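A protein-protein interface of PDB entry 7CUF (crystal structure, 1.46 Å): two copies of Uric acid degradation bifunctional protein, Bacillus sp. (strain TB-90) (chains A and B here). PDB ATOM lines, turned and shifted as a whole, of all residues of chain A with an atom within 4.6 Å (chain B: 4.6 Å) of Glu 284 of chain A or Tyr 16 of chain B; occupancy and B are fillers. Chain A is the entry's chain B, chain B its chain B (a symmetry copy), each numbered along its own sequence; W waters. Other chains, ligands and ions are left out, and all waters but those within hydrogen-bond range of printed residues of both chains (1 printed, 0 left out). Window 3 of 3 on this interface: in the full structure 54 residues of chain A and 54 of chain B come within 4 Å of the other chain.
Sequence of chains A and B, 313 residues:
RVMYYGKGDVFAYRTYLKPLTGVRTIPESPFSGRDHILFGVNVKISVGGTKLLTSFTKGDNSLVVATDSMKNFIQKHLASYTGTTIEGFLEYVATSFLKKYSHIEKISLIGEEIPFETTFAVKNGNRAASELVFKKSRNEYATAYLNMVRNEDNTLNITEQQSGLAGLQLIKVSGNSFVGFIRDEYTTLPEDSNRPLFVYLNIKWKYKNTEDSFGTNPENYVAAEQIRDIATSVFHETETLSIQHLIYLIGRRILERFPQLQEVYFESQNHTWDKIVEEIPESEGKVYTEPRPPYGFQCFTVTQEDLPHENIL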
ATOM      1  N   VAL A 173      29.291  -8.906 -33.787  1.00  0.00           N
ATOM      2  CA  VAL A 173      29.184  -9.470 -32.432  1.00  0.00           C
ATOM      3  C   VAL A 173      30.332  -9.053 -31.526  1.00  0.00           C
ATOM      4  O   VAL A 173      30.179  -9.083 -30.303  1.00  0.00           O
ATOM      5  CB  VAL A 173      29.016 -11.001 -32.496  1.00  0.00           C
ATOM      6  CG1 VAL A 173      27.680 -11.313 -33.185  1.00  0.00           C
ATOM      7  CG2 VAL A 173      30.230 -11.642 -33.195  1.00  0.00           C
ATOM      8  N   SER A 283      32.670 -21.490 -22.379  1.00  0.00           N
ATOM      9  CA  SER A 283      32.136 -20.933 -23.609  1.00  0.00           C
ATOM     10  C   SER A 283      32.632 -19.500 -23.756  1.00  0.00           C
ATOM     11  O   SER A 283      32.961 -18.840 -22.764  1.00  0.00           O
ATOM     12  CB  SER A 283      30.595 -20.961 -23.622  1.00  0.00           C
ATOM     13  N   GLU A 284      32.701 -19.040 -25.004  1.00  0.00           N
ATOM     14  CA  GLU A 284      32.950 -17.640 -25.311  1.00  0.00           C
ATOM     15  C   GLU A 284      31.654 -16.871 -25.541  1.00  0.00           C
ATOM     16  O   GLU A 284      31.696 -15.712 -25.973  1.00  0.00           O
ATOM     17  CB  GLU A 284      33.856 -17.514 -26.533  1.00  0.00           C
ATOM     18  N   GLY A 285      30.502 -17.502 -25.261  1.00  0.00           N
ATOM     19  CA  GLY A 285      29.217 -16.876 -25.486  1.00  0.00           C
ATOM     20  C   GLY A 285      28.786 -15.961 -24.343  1.00  0.00           C
ATOM     21  O   GLY A 285      29.327 -15.975 -23.236  1.00  0.00           O
ATOM     22  N   LYS A 286      27.754 -15.176 -24.638  1.00  0.00           N
ATOM     23  CA  LYS A 286      27.156 -14.227 -23.716  1.00  0.00           C
ATOM     24  C   LYS A 286      25.668 -14.217 -24.052  1.00  0.00           C
ATOM     25  O   LYS A 286      25.260 -14.762 -25.094  1.00  0.00           O
ATOM     26  CB  LYS A 286      27.766 -12.852 -23.946  1.00  0.00           C
ATOM     27  CG  LYS A 286      29.294 -12.778 -23.704  1.00  0.00           C
ATOM     28  CD  LYS A 286      29.748 -11.328 -23.687  1.00  0.00           C
ATOM     29  N   ARG B  14      22.052 -15.129 -27.838  1.00  0.00           N
ATOM     30  CA  ARG B  14      23.128 -15.945 -27.290  1.00  0.00           C
ATOM     31  C   ARG B  14      24.169 -16.053 -28.393  1.00  0.00           C
ATOM     32  O   ARG B  14      23.816 -16.295 -29.553  1.00  0.00           O
ATOM     33  CB  ARG B  14      22.596 -17.318 -26.837  1.00  0.00           C
ATOM     34  CG  ARG B  14      23.617 -18.442 -26.720  1.00  0.00           C
ATOM     35  CD  ARG B  14      24.329 -18.447 -25.390  1.00  0.00           C
ATOM     36  NE  ARG B  14      25.432 -19.391 -25.446  1.00  0.00           N
ATOM     37  CZ  ARG B  14      25.433 -20.626 -24.945  1.00  0.00           C
ATOM     38  NH1 ARG B  14      24.378 -21.092 -24.305  1.00  0.00           N
ATOM     39  NH2 ARG B  14      26.504 -21.392 -25.105  1.00  0.00           N
ATOM     40  N   THR B  15      25.431 -15.851 -28.049  1.00  0.00           N
ATOM     41  CA  THR B  15      26.491 -16.101 -29.002  1.00  0.00           C
ATOM     42  C   THR B  15      27.100 -17.460 -28.716  1.00  0.00           C
ATOM     43  O   THR B  15      27.068 -17.957 -27.579  1.00  0.00           O
ATOM     44  CB  THR B  15      27.529 -14.997 -29.003  1.00  0.00           C
ATOM     45  OG1 THR B  15      28.012 -14.794 -27.659  1.00  0.00           O
ATOM     46  CG2 THR B  15      26.907 -13.690 -29.505  1.00  0.00           C
ATOM     47  N   TYR B  16      27.589 -18.090 -29.786  1.00  0.00           N
ATOM     48  CA  TYR B  16      28.299 -19.365 -29.703  1.00  0.00           C
ATOM     49  C   TYR B  16      27.513 -20.432 -28.947  1.00  0.00           C
ATOM     50  O   TYR B  16      28.016 -21.084 -28.035  1.00  0.00           O
ATOM     51  CB  TYR B  16      29.736 -19.174 -29.181  1.00  0.00           C
ATOM     52  CG  TYR B  16      30.435 -18.100 -29.988  1.00  0.00           C
ATOM     53  CD1 TYR B  16      30.864 -18.360 -31.280  1.00  0.00           C
ATOM     54  CD2 TYR B  16      30.609 -16.817 -29.490  1.00  0.00           C
ATOM     55  CE1 TYR B  16      31.466 -17.377 -32.056  1.00  0.00           C
ATOM     56  CE2 TYR B  16      31.203 -15.823 -30.254  1.00  0.00           C
ATOM     57  CZ  TYR B  16      31.623 -16.107 -31.545  1.00  0.00           C
ATOM     58  OH  TYR B  16      32.201 -15.123 -32.324  1.00  0.00           O
ATOM     59  N   LEU B  17      26.272 -20.659 -29.391  1.00  0.00           N
ATOM     60  CA  LEU B  17      25.567 -21.874 -29.016  1.00  0.00           C
ATOM     61  C   LEU B  17      26.258 -23.060 -29.684  1.00  0.00           C
ATOM     62  O   LEU B  17      26.935 -22.919 -30.717  1.00  0.00           O
ATOM     63  CB  LEU B  17      24.100 -21.788 -29.460  1.00  0.00           C
ATOM     64  CG  LEU B  17      23.135 -22.774 -28.812  1.00  0.00           C
ATOM     65  CD1 LEU B  17      22.865 -22.312 -27.381  1.00  0.00           C
ATOM     66  CD2 LEU B  17      21.829 -22.885 -29.586  1.00  0.00           C
ATOM     67  N   LYS B  18      26.108 -24.245 -29.097  1.00  0.00           N
ATOM     68  CA  LYS B  18      26.646 -25.434 -29.735  1.00  0.00           C
ATOM     69  C   LYS B  18      26.073 -25.574 -31.149  1.00  0.00           C
ATOM     70  O   LYS B  18      24.857 -25.476 -31.334  1.00  0.00           O
ATOM     71  CB  LYS B  18      26.251 -26.676 -28.912  1.00  0.00           C
ATOM     72  CG  LYS B  18      26.850 -27.981 -29.402  1.00  0.00           C
ATOM     73  CD  LYS B  18      26.359 -29.146 -28.540  1.00  0.00           C
ATOM     74  CE  LYS B  18      27.016 -30.461 -28.966  1.00  0.00           C
ATOM     75  NZ  LYS B  18      26.104 -31.439 -29.634  1.00  0.00           N
ATOM     76  N   HIS B  36      25.406 -21.250 -35.417  1.00  0.00           N
ATOM     77  CA  HIS B  36      25.019 -20.769 -34.093  1.00  0.00           C
ATOM     78  C   HIS B  36      26.029 -19.794 -33.518  1.00  0.00           C
ATOM     79  O   HIS B  36      26.149 -19.676 -32.293  1.00  0.00           O
ATOM     80  CB  HIS B  36      24.755 -21.917 -33.117  1.00  0.00           C
ATOM     81  CG  HIS B  36      23.472 -22.639 -33.379  1.00  0.00           C
ATOM     82  ND1 HIS B  36      23.221 -23.915 -32.911  1.00  0.00           N
ATOM     83  CD2 HIS B  36      22.340 -22.241 -34.015  1.00  0.00           C
ATOM     84  CE1 HIS B  36      22.000 -24.278 -33.293  1.00  0.00           C
ATOM     85  NE2 HIS B  36      21.442 -23.280 -33.954  1.00  0.00           N
ATOM     86  N   ILE B  37      26.783 -19.086 -34.371  1.00  0.00           N
ATOM     87  CA  ILE B  37      27.535 -17.928 -33.883  1.00  0.00           C
ATOM     88  C   ILE B  37      26.600 -16.936 -33.193  1.00  0.00           C
ATOM     89  O   ILE B  37      26.952 -16.342 -32.170  1.00  0.00           O
ATOM     90  CB  ILE B  37      28.300 -17.249 -35.025  1.00  0.00           C
ATOM     91  CG1 ILE B  37      29.357 -18.215 -35.559  1.00  0.00           C
ATOM     92  CG2 ILE B  37      28.941 -15.942 -34.523  1.00  0.00           C
ATOM     93  CD1 ILE B  37      29.950 -17.814 -36.880  1.00  0.00           C
ATOM     94  N   GLU B 131      32.521 -14.131 -40.008  1.00  0.00           N
ATOM     95  CA  GLU B 131      32.224 -14.794 -38.740  1.00  0.00           C
ATOM     96  C   GLU B 131      31.743 -13.815 -37.677  1.00  0.00           C
ATOM     97  O   GLU B 131      31.415 -14.243 -36.549  1.00  0.00           O
ATOM     98  CB  GLU B 131      33.475 -15.547 -38.241  1.00  0.00           C
ATOM     99  CG  GLU B 131      34.554 -14.685 -37.539  1.00  0.00           C
ATOM    100  CD  GLU B 131      35.506 -14.009 -38.511  1.00  0.00           C
ATOM    101  OE1 GLU B 131      35.225 -13.988 -39.730  1.00  0.00           O
ATOM    102  OE2 GLU B 131      36.572 -13.521 -38.051  1.00  0.00           O
HETATM  103  O   HOH W   1      30.011 -13.133 -27.631  1.00  0.00           O
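N of Lys 286 of chain A sits at hydrogen-bond distance from OG1 of Thr 15 of chain B.
N of Tyr 16 of chain B lies within hydrogen-bond range of O of His 36 of chain B, at 3.3 Å. The guanidinium group (NH2) of Arg 14 of chain B sits at hydrogen-bond distance from the backbone carbonyl oxygen (O) of Tyr 16 of chain B (3.3 Å). O of Ile 37 of chain B lies within hydrogen-bond range of N of Tyr 16 of chain B, at 3.0 Å.
Among the printed residues, pairs that only touch across the chains: Glu 284 of chain A with Tyr 16 of chain B, Gly 285 of chain A with Thr 15 of chain B and Lys 286 of chain A with Arg 14 of chain B.
Of the printed residues of chain B, Glu 284 of chain A touches Tyr 16 (3.8 Å). Of the printed residues of chain B, Gly 285 of chain A touches Thr 15 (3.2 Å). Of the printed residues of chain B, Lys 286 of chain A touches Arg 14 and Thr 15. Of chain A, only Glu 284 (3.8 Å) comes within 4 Å of Tyr 16 of chain B. His 36 of chain B touches none of the printed residues of chain A. The nearest residue of chain B that does not touch Glu 284 of chain A is Thr 15 of chain B (4.2 Å).
Of the 5 printed residues of chain A, 3 touch a printed residue of chain B. Printed residues of chain B that touch a printed residue of chain A: Arg 14, Thr 15 and Tyr 16. Hydrophobic or aromatic side chains of chain B within 4 Å of the printed part of chain A: Tyr 16. Among the printed residues, 4 pairs touch across the chains. Among the printed residues, no Asp or Glu carboxylate lies within 4 Å of a Lys or Arg side-chain nitrogen of the other chain.
No position is printed for both chains. Of the 4 pairs that touch across the chains among the printed residues, none has its exchanged pair printed and touching as well.
Water W1 lies within hydrogen-bond range of the side-chain hydroxyl (OG1) of Thr 15 of chain B (2.6 Å) and the backbone carbonyl oxygen (O) of Glu 284 of chain A (3.5 Å).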
